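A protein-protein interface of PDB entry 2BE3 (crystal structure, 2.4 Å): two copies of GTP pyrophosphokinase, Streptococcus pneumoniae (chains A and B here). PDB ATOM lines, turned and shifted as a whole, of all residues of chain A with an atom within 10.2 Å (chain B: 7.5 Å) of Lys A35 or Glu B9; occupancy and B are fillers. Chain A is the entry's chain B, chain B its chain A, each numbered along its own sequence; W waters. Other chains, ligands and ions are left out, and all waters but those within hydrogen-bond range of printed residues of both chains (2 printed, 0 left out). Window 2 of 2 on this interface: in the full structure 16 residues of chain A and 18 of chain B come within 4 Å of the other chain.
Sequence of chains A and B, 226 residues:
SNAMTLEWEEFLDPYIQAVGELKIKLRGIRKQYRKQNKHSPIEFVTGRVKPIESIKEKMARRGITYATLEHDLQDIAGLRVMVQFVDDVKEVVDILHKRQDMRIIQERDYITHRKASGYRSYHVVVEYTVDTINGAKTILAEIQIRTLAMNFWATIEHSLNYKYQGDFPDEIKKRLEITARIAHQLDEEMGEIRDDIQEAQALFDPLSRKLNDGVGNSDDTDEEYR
Of the 14 printed residues of chain A, 2 touch a printed residue of chain B.
Along chain A the printed residues that touch a printed residue of chain B span positions 32 to 35.
Among the printed residues, Asp or Glu carboxylates within 4 Å of a Lys or Arg side-chain nitrogen of the other chain: Lys A35 with Asp B13.
O of Gln A32 sits at hydrogen-bond distance from NE2 of Gln A36 (3.1 Å).
No position is printed for both chains.
Of the 4 pairs that touch across the chains among the printed residues, none has its exchanged pair printed and touching as well.
Lys A35 touches Glu B9 (CE to CG, 3.9 Å).
NZ of Lys A35 touches CD1 of Ile B16, 3.8 Å away.
Of the printed residues of chain A, Gln B17 touches Gln A32 (2.7 Å).
Of the printed residues of chain B, Gln A32 touches Gln B17.
Of the printed residues of chain A, Ile B16 touches Lys A35.
Met B4 touches none of the printed residues of chain A.
Pro B14 touches none of the printed residues of chain A.
The nearest residue of chain B that does not touch Lys A35 is Leu B12 (5.8 Å).
Water W1 lies within hydrogen-bond range of the side-chain amide oxygen (OE1) of Gln B17 (2.6 Å) and the side-chain amide nitrogen (NE2) of Gln A32 (3.3 Å).
Water W2 bridges the side-chain carboxylate of Asp B13 (2.8 Å) and the side-chain amide nitrogen of Gln A36 (3.1 Å).
The side-chain amino group of Lys A35 is in salt-bridge range of the side-chain carboxylate of Asp B13.
The side-chain amide oxygen (OE1) of Gln B17 sits at hydrogen-bond distance from the side-chain amide nitrogen (NE2) of Gln A32 (2.7 Å).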
ATOM      1  N   ARG A  27      25.072  21.353   4.354  1.00  0.00           N
ATOM      2  CA  ARG A  27      25.358  22.775   4.497  1.00  0.00           C
ATOM      3  C   ARG A  27      24.865  23.400   5.804  1.00  0.00           C
ATOM      4  O   ARG A  27      25.491  24.334   6.301  1.00  0.00           O
ATOM      5  CB  ARG A  27      24.808  23.544   3.307  1.00  0.00           C
ATOM      6  CG  ARG A  27      25.720  23.436   2.088  1.00  0.00           C
ATOM      7  CD  ARG A  27      25.001  23.875   0.829  1.00  0.00           C
ATOM      8  NE  ARG A  27      25.768  23.525  -0.363  1.00  0.00           N
ATOM      9  CZ  ARG A  27      25.299  23.528  -1.608  1.00  0.00           C
ATOM     10  NH1 ARG A  27      24.039  23.852  -1.859  1.00  0.00           N
ATOM     11  NH2 ARG A  27      26.096  23.195  -2.606  1.00  0.00           N
ATOM     12  N   GLY A  28      23.771  22.893   6.363  1.00  0.00           N
ATOM     13  CA  GLY A  28      23.222  23.413   7.603  1.00  0.00           C
ATOM     14  C   GLY A  28      23.985  22.948   8.835  1.00  0.00           C
ATOM     15  O   GLY A  28      23.894  23.564   9.894  1.00  0.00           O
ATOM     16  N   ILE A  29      24.713  21.842   8.720  1.00  0.00           N
ATOM     17  CA  ILE A  29      25.651  21.448   9.761  1.00  0.00           C
ATOM     18  C   ILE A  29      26.647  22.584   9.957  1.00  0.00           C
ATOM     19  O   ILE A  29      26.872  23.006  11.080  1.00  0.00           O
ATOM     20  CB  ILE A  29      26.424  20.164   9.397  1.00  0.00           C
ATOM     21  CG1 ILE A  29      25.510  18.956   9.494  1.00  0.00           C
ATOM     22  CG2 ILE A  29      27.649  19.983  10.295  1.00  0.00           C
ATOM     23  CD1 ILE A  29      26.079  17.749   8.807  1.00  0.00           C
ATOM     24  N   ARG A  30      27.238  23.066   8.862  1.00  0.00           N
ATOM     25  CA  ARG A  30      28.202  24.154   8.918  1.00  0.00           C
ATOM     26  C   ARG A  30      27.608  25.388   9.584  1.00  0.00           C
ATOM     27  O   ARG A  30      28.218  25.948  10.500  1.00  0.00           O
ATOM     28  CB  ARG A  30      28.709  24.519   7.527  1.00  0.00           C
ATOM     29  CG  ARG A  30      29.541  25.771   7.552  1.00  0.00           C
ATOM     30  CD  ARG A  30      30.282  26.045   6.248  1.00  0.00           C
ATOM     31  NE  ARG A  30      30.836  27.409   6.254  1.00  0.00           N
ATOM     32  CZ  ARG A  30      32.006  27.777   6.785  1.00  0.00           C
ATOM     33  NH1 ARG A  30      32.825  26.892   7.364  1.00  0.00           N
ATOM     34  NH2 ARG A  30      32.361  29.047   6.726  1.00  0.00           N
ATOM     35  N   LYS A  31      26.418  25.805   9.135  1.00  0.00           N
ATOM     36  CA  LYS A  31      25.770  26.999   9.685  1.00  0.00           C
ATOM     37  C   LYS A  31      25.521  26.843  11.185  1.00  0.00           C
ATOM     38  O   LYS A  31      25.556  27.820  11.926  1.00  0.00           O
ATOM     39  CB  LYS A  31      24.460  27.335   8.954  1.00  0.00           C
ATOM     40  CG  LYS A  31      24.563  27.250   7.436  1.00  0.00           C
ATOM     41  CD  LYS A  31      23.626  28.211   6.714  1.00  0.00           C
ATOM     42  CE  LYS A  31      22.182  27.720   6.673  1.00  0.00           C
ATOM     43  NZ  LYS A  31      22.001  26.509   5.821  1.00  0.00           N
ATOM     44  N   GLN A  32      25.286  25.612  11.626  1.00  0.00           N
ATOM     45  CA  GLN A  32      25.050  25.335  13.034  1.00  0.00           C
ATOM     46  C   GLN A  32      26.305  25.472  13.879  1.00  0.00           C
ATOM     47  O   GLN A  32      26.226  25.827  15.044  1.00  0.00           O
ATOM     48  CB  GLN A  32      24.438  23.943  13.217  1.00  0.00           C
ATOM     49  CG  GLN A  32      22.940  23.894  12.993  1.00  0.00           C
ATOM     50  CD  GLN A  32      22.362  22.503  13.163  1.00  0.00           C
ATOM     51  OE1 GLN A  32      22.963  21.635  13.774  1.00  0.00           O
ATOM     52  NE2 GLN A  32      21.183  22.293  12.619  1.00  0.00           N
ATOM     53  N   TYR A  33      27.459  25.166  13.299  1.00  0.00           N
ATOM     54  CA  TYR A  33      28.723  25.305  14.014  1.00  0.00           C
ATOM     55  C   TYR A  33      29.113  26.769  14.133  1.00  0.00           C
ATOM     56  O   TYR A  33      29.537  27.214  15.200  1.00  0.00           O
ATOM     57  CB  TYR A  33      29.831  24.523  13.321  1.00  0.00           C
ATOM     58  CG  TYR A  33      29.955  23.081  13.775  1.00  0.00           C
ATOM     59  CD1 TYR A  33      29.323  22.054  13.081  1.00  0.00           C
ATOM     60  CD2 TYR A  33      30.721  22.746  14.885  1.00  0.00           C
ATOM     61  CE1 TYR A  33      29.441  20.740  13.486  1.00  0.00           C
ATOM     62  CE2 TYR A  33      30.846  21.435  15.298  1.00  0.00           C
ATOM     63  CZ  TYR A  33      30.201  20.437  14.598  1.00  0.00           C
ATOM     64  OH  TYR A  33      30.324  19.132  15.007  1.00  0.00           O
ATOM     65  N   ARG A  34      28.957  27.513  13.039  1.00  0.00           N
ATOM     66  CA  ARG A  34      29.299  28.934  13.007  1.00  0.00           C
ATOM     67  C   ARG A  34      28.395  29.763  13.923  1.00  0.00           C
ATOM     68  O   ARG A  34      28.877  30.634  14.648  1.00  0.00           O
ATOM     69  CB  ARG A  34      29.241  29.483  11.581  1.00  0.00           C
ATOM     70  CG  ARG A  34      30.200  28.832  10.604  1.00  0.00           C
ATOM     71  CD  ARG A  34      30.437  29.728   9.424  1.00  0.00           C
ATOM     72  NE  ARG A  34      31.474  30.705   9.749  1.00  0.00           N
ATOM     73  CZ  ARG A  34      31.258  31.979  10.089  1.00  0.00           C
ATOM     74  NH1 ARG A  34      32.291  32.768  10.374  1.00  0.00           N
ATOM     75  NH2 ARG A  34      30.021  32.475  10.141  1.00  0.00           N
ATOM     76  N   LYS A  35      27.093  29.482  13.896  1.00  0.00           N
ATOM     77  CA  LYS A  35      26.128  30.201  14.727  1.00  0.00           C
ATOM     78  C   LYS A  35      26.423  30.017  16.222  1.00  0.00           C
ATOM     79  O   LYS A  35      26.191  30.930  17.020  1.00  0.00           O
ATOM     80  CB  LYS A  35      24.696  29.760  14.409  1.00  0.00           C
ATOM     81  CG  LYS A  35      23.639  30.831  14.672  1.00  0.00           C
ATOM     82  CD  LYS A  35      22.226  30.270  14.648  1.00  0.00           C
ATOM     83  CE  LYS A  35      21.206  31.365  14.962  1.00  0.00           C
ATOM     84  NZ  LYS A  35      19.817  30.814  15.046  1.00  0.00           N
ATOM     85  N   GLN A  36      26.940  28.840  16.585  1.00  0.00           N
ATOM     86  CA  GLN A  36      27.320  28.514  17.968  1.00  0.00           C
ATOM     87  C   GLN A  36      28.819  28.756  18.210  1.00  0.00           C
ATOM     88  O   GLN A  36      29.419  28.179  19.122  1.00  0.00           O
ATOM     89  CB  GLN A  36      26.913  27.069  18.307  1.00  0.00           C
ATOM     90  CG  GLN A  36      25.391  26.868  18.446  1.00  0.00           C
ATOM     91  CD  GLN A  36      24.927  25.437  18.127  1.00  0.00           C
ATOM     92  OE1 GLN A  36      25.399  24.466  18.727  1.00  0.00           O
ATOM     93  NE2 GLN A  36      23.987  25.311  17.181  1.00  0.00           N
ATOM     94  N   ASN A  37      29.401  29.625  17.380  1.00  0.00           N
ATOM     95  CA  ASN A  37      30.807  30.025  17.455  1.00  0.00           C
ATOM     96  C   ASN A  37      31.781  28.891  17.728  1.00  0.00           C
ATOM     97  O   ASN A  37      32.418  28.864  18.786  1.00  0.00           O
ATOM     98  CB  ASN A  37      31.001  31.125  18.503  1.00  0.00           C
ATOM     99  CG  ASN A  37      30.225  32.382  18.177  1.00  0.00           C
ATOM    100  OD1 ASN A  37      30.624  33.163  17.307  1.00  0.00           O
ATOM    101  ND2 ASN A  37      29.108  32.591  18.880  1.00  0.00           N
ATOM    102  N   LYS A  38      31.891  27.959  16.779  1.00  0.00           N
ATOM    103  CA  LYS A  38      32.854  26.852  16.860  1.00  0.00           C
ATOM    104  C   LYS A  38      33.412  26.588  15.463  1.00  0.00           C
ATOM    105  O   LYS A  38      32.769  26.939  14.466  1.00  0.00           O
ATOM    106  CB  LYS A  38      32.189  25.578  17.404  1.00  0.00           C
ATOM    107  CG  LYS A  38      31.448  25.725  18.732  1.00  0.00           C
ATOM    108  CD  LYS A  38      31.034  24.377  19.298  1.00  0.00           C
ATOM    109  CE  LYS A  38      29.970  24.541  20.389  1.00  0.00           C
ATOM    110  NZ  LYS A  38      28.584  24.638  19.820  1.00  0.00           N
ATOM    111  N   HIS A  39      34.605  25.984  15.386  1.00  0.00           N
ATOM    112  CA  HIS A  39      35.171  25.536  14.101  1.00  0.00           C
ATOM    113  C   HIS A  39      34.177  24.566  13.496  1.00  0.00           C
ATOM    114  O   HIS A  39      33.777  23.586  14.146  1.00  0.00           O
ATOM    115  CB  HIS A  39      36.528  24.846  14.290  1.00  0.00           C
ATOM    116  CG  HIS A  39      37.131  24.286  13.026  1.00  0.00           C
ATOM    117  ND1 HIS A  39      37.570  25.084  11.989  1.00  0.00           N
ATOM    118  CD2 HIS A  39      37.426  23.009  12.665  1.00  0.00           C
ATOM    119  CE1 HIS A  39      38.079  24.321  11.033  1.00  0.00           C
ATOM    120  NE2 HIS A  39      38.013  23.059  11.421  1.00  0.00           N
ATOM    121  N   SER A  40      33.745  24.879  12.281  1.00  0.00           N
ATOM    122  CA  SER A  40      32.965  23.959  11.496  1.00  0.00           C
ATOM    123  C   SER A  40      33.919  22.959  10.891  1.00  0.00           C
ATOM    124  O   SER A  40      34.847  23.359  10.190  1.00  0.00           O
ATOM    125  CB  SER A  40      32.229  24.683  10.379  1.00  0.00           C
ATOM    126  OG  SER A  40      31.445  23.768   9.646  1.00  0.00           O
ATOM    127  N   MET B   4      15.837  39.080  22.681  1.00  0.00           N
ATOM    128  CA  MET B   4      16.662  38.193  21.801  1.00  0.00           C
ATOM    129  C   MET B   4      18.016  37.813  22.445  1.00  0.00           C
ATOM    130  O   MET B   4      19.077  38.328  22.073  1.00  0.00           O
ATOM    131  CB  MET B   4      16.828  38.821  20.401  1.00  0.00           C
ATOM    132  CG  MET B   4      17.682  38.003  19.403  1.00  0.00           C
ATOM    133  SD  MET B   4      16.979  36.210  18.881  1.00  0.00           S
ATOM    134  CE  MET B   4      15.888  36.747  17.208  1.00  0.00           C
ATOM    135  N   THR B   5      17.961  36.896  23.409  1.00  0.00           N
ATOM    136  CA  THR B   5      19.146  36.473  24.161  1.00  0.00           C
ATOM    137  C   THR B   5      19.836  35.244  23.548  1.00  0.00           C
ATOM    138  O   THR B   5      19.415  34.719  22.514  1.00  0.00           O
ATOM    139  CB  THR B   5      18.802  36.194  25.668  1.00  0.00           C
ATOM    140  OG1 THR B   5      17.990  35.021  25.786  1.00  0.00           O
ATOM    141  CG2 THR B   5      18.081  37.381  26.316  1.00  0.00           C
ATOM    142  N   LEU B   6      20.897  34.787  24.208  1.00  0.00           N
ATOM    143  CA  LEU B   6      21.565  33.536  23.845  1.00  0.00           C
ATOM    144  C   LEU B   6      20.714  32.269  24.053  1.00  0.00           C
ATOM    145  O   LEU B   6      20.754  31.366  23.213  1.00  0.00           O
ATOM    146  CB  LEU B   6      22.908  33.386  24.583  1.00  0.00           C
ATOM    147  CG  LEU B   6      23.867  32.325  24.014  1.00  0.00           C
ATOM    148  CD1 LEU B   6      24.644  32.891  22.799  1.00  0.00           C
ATOM    149  CD2 LEU B   6      24.816  31.790  25.083  1.00  0.00           C
ATOM    150  N   GLU B   7      19.961  32.214  25.150  1.00  0.00           N
ATOM    151  CA  GLU B   7      19.109  31.055  25.435  1.00  0.00           C
ATOM    152  C   GLU B   7      17.893  30.982  24.500  1.00  0.00           C
ATOM    153  O   GLU B   7      17.454  29.887  24.140  1.00  0.00           O
ATOM    154  CB  GLU B   7      18.709  30.982  26.919  1.00  0.00           C
ATOM    155  CG  GLU B   7      18.506  32.329  27.617  1.00  0.00           C
ATOM    156  CD  GLU B   7      19.815  33.011  28.005  1.00  0.00           C
ATOM    157  OE1 GLU B   7      20.745  32.328  28.490  1.00  0.00           O
ATOM    158  OE2 GLU B   7      19.910  34.241  27.819  1.00  0.00           O
ATOM    159  N   TRP B   8      17.378  32.145  24.097  1.00  0.00           N
ATOM    160  CA  TRP B   8      16.307  32.233  23.097  1.00  0.00           C
ATOM    161  C   TRP B   8      16.757  31.759  21.727  1.00  0.00           C
ATOM    162  O   TRP B   8      15.979  31.182  20.989  1.00  0.00           O
ATOM    163  CB  TRP B   8      15.749  33.650  22.968  1.00  0.00           C
ATOM    164  CG  TRP B   8      14.600  33.919  23.889  1.00  0.00           C
ATOM    165  CD1 TRP B   8      14.574  34.819  24.909  1.00  0.00           C
ATOM    166  CD2 TRP B   8      13.314  33.260  23.902  1.00  0.00           C
ATOM    167  NE1 TRP B   8      13.362  34.776  25.548  1.00  0.00           N
ATOM    168  CE2 TRP B   8      12.570  33.826  24.959  1.00  0.00           C
ATOM    169  CE3 TRP B   8      12.720  32.249  23.123  1.00  0.00           C
ATOM    170  CZ2 TRP B   8      11.256  33.432  25.254  1.00  0.00           C
ATOM    171  CZ3 TRP B   8      11.421  31.854  23.423  1.00  0.00           C
ATOM    172  CH2 TRP B   8      10.702  32.454  24.472  1.00  0.00           C
ATOM    173  N   GLU B   9      18.022  32.009  21.412  1.00  0.00           N
ATOM    174  CA  GLU B   9      18.637  31.657  20.139  1.00  0.00           C
ATOM    175  C   GLU B   9      18.867  30.147  20.065  1.00  0.00           C
ATOM    176  O   GLU B   9      18.593  29.509  19.057  1.00  0.00           O
ATOM    177  CB  GLU B   9      19.971  32.398  20.020  1.00  0.00           C
ATOM    178  CG  GLU B   9      20.541  32.444  18.635  1.00  0.00           C
ATOM    179  CD  GLU B   9      21.859  33.239  18.570  1.00  0.00           C
ATOM    180  OE1 GLU B   9      21.896  34.291  17.868  1.00  0.00           O
ATOM    181  OE2 GLU B   9      22.837  32.816  19.243  1.00  0.00           O
ATOM    182  N   GLU B  10      19.359  29.580  21.156  1.00  0.00           N
ATOM    183  CA  GLU B  10      19.549  28.150  21.244  1.00  0.00           C
ATOM    184  C   GLU B  10      18.228  27.397  21.199  1.00  0.00           C
ATOM    185  O   GLU B  10      18.161  26.289  20.658  1.00  0.00           O
ATOM    186  CB  GLU B  10      20.315  27.790  22.509  1.00  0.00           C
ATOM    187  CG  GLU B  10      21.796  28.146  22.414  1.00  0.00           C
ATOM    188  CD  GLU B  10      22.559  27.903  23.732  1.00  0.00           C
ATOM    189  OE1 GLU B  10      21.991  27.325  24.709  1.00  0.00           O
ATOM    190  OE2 GLU B  10      23.747  28.296  23.778  1.00  0.00           O
ATOM    191  N   PHE B  11      17.179  28.008  21.751  1.00  0.00           N
ATOM    192  CA  PHE B  11      15.874  27.373  21.768  1.00  0.00           C
ATOM    193  C   PHE B  11      15.212  27.394  20.384  1.00  0.00           C
ATOM    194  O   PHE B  11      14.599  26.414  19.964  1.00  0.00           O
ATOM    195  CB  PHE B  11      14.964  28.029  22.810  1.00  0.00           C
ATOM    196  CG  PHE B  11      13.564  27.503  22.785  1.00  0.00           C
ATOM    197  CD1 PHE B  11      13.263  26.260  23.354  1.00  0.00           C
ATOM    198  CD2 PHE B  11      12.547  28.226  22.175  1.00  0.00           C
ATOM    199  CE1 PHE B  11      11.974  25.768  23.324  1.00  0.00           C
ATOM    200  CE2 PHE B  11      11.250  27.723  22.127  1.00  0.00           C
ATOM    201  CZ  PHE B  11      10.966  26.511  22.701  1.00  0.00           C
ATOM    202  N   LEU B  12      15.349  28.508  19.687  1.00  0.00           N
ATOM    203  CA  LEU B  12      14.619  28.738  18.444  1.00  0.00           C
ATOM    204  C   LEU B  12      15.221  28.074  17.220  1.00  0.00           C
ATOM    205  O   LEU B  12      14.501  27.762  16.270  1.00  0.00           O
ATOM    206  CB  LEU B  12      14.471  30.235  18.179  1.00  0.00           C
ATOM    207  CG  LEU B  12      13.520  30.929  19.138  1.00  0.00           C
ATOM    208  CD1 LEU B  12      13.511  32.410  18.844  1.00  0.00           C
ATOM    209  CD2 LEU B  12      12.120  30.308  19.099  1.00  0.00           C
ATOM    210  N   ASP B  13      16.530  27.845  17.253  1.00  0.00           N
ATOM    211  CA  ASP B  13      17.250  27.221  16.136  1.00  0.00           C
ATOM    212  C   ASP B  13      16.594  26.005  15.490  1.00  0.00           C
ATOM    213  O   ASP B  13      16.435  25.982  14.281  1.00  0.00           O
ATOM    214  CB  ASP B  13      18.684  26.893  16.528  1.00  0.00           C
ATOM    215  CG  ASP B  13      19.645  27.866  15.967  1.00  0.00           C
ATOM    216  OD1 ASP B  13      20.521  28.360  16.731  1.00  0.00           O
ATOM    217  OD2 ASP B  13      19.519  28.169  14.741  1.00  0.00           O
ATOM    218  N   PRO B  14      16.251  24.976  16.284  1.00  0.00           N
ATOM    219  CA  PRO B  14      15.537  23.845  15.672  1.00  0.00           C
ATOM    220  C   PRO B  14      14.293  24.268  14.880  1.00  0.00           C
ATOM    221  O   PRO B  14      14.048  23.717  13.816  1.00  0.00           O
ATOM    222  CB  PRO B  14      15.154  22.959  16.867  1.00  0.00           C
ATOM    223  CG  PRO B  14      16.066  23.370  17.951  1.00  0.00           C
ATOM    224  CD  PRO B  14      16.541  24.762  17.713  1.00  0.00           C
ATOM    225  N   ILE B  16      13.718  27.444  13.482  1.00  0.00           N
ATOM    226  CA  ILE B  16      14.233  28.076  12.276  1.00  0.00           C
ATOM    227  C   ILE B  16      14.653  26.990  11.246  1.00  0.00           C
ATOM    228  O   ILE B  16      14.261  27.037  10.075  1.00  0.00           O
ATOM    229  CB  ILE B  16      15.430  29.044  12.620  1.00  0.00           C
ATOM    230  CG1 ILE B  16      14.954  30.203  13.500  1.00  0.00           C
ATOM    231  CG2 ILE B  16      16.123  29.619  11.373  1.00  0.00           C
ATOM    232  CD1 ILE B  16      16.092  31.009  14.175  1.00  0.00           C
ATOM    233  N   GLN B  17      15.432  26.010  11.693  1.00  0.00           N
ATOM    234  CA  GLN B  17      15.813  24.884  10.855  1.00  0.00           C
ATOM    235  C   GLN B  17      14.603  24.132  10.260  1.00  0.00           C
ATOM    236  O   GLN B  17      14.567  23.912   9.041  1.00  0.00           O
ATOM    237  CB  GLN B  17      16.697  23.913  11.637  1.00  0.00           C
ATOM    238  CG  GLN B  17      17.383  22.927  10.759  1.00  0.00           C
ATOM    239  CD  GLN B  17      18.136  21.891  11.530  1.00  0.00           C
ATOM    240  OE1 GLN B  17      18.466  22.083  12.696  1.00  0.00           O
ATOM    241  NE2 GLN B  17      18.390  20.759  10.895  1.00  0.00           N
ATOM    242  N   ILE B  52       9.675  36.030  19.367  1.00  0.00           N
ATOM    243  CA  ILE B  52       9.818  35.881  20.816  1.00  0.00           C
ATOM    244  C   ILE B  52       8.741  36.608  21.625  1.00  0.00           C
ATOM    245  O   ILE B  52       8.244  36.055  22.627  1.00  0.00           O
ATOM    246  CB  ILE B  52      11.233  36.362  21.291  1.00  0.00           C
ATOM    247  CG1 ILE B  52      12.330  35.465  20.708  1.00  0.00           C
ATOM    248  CG2 ILE B  52      11.344  36.409  22.813  1.00  0.00           C
ATOM    249  CD1 ILE B  52      13.706  36.119  20.732  1.00  0.00           C
HETATM  250  O   HOH W   1      19.037  23.648  14.726  1.00  0.00           O
HETATM  251  O   HOH W   2      21.839  26.954  18.726  1.00  0.00           O
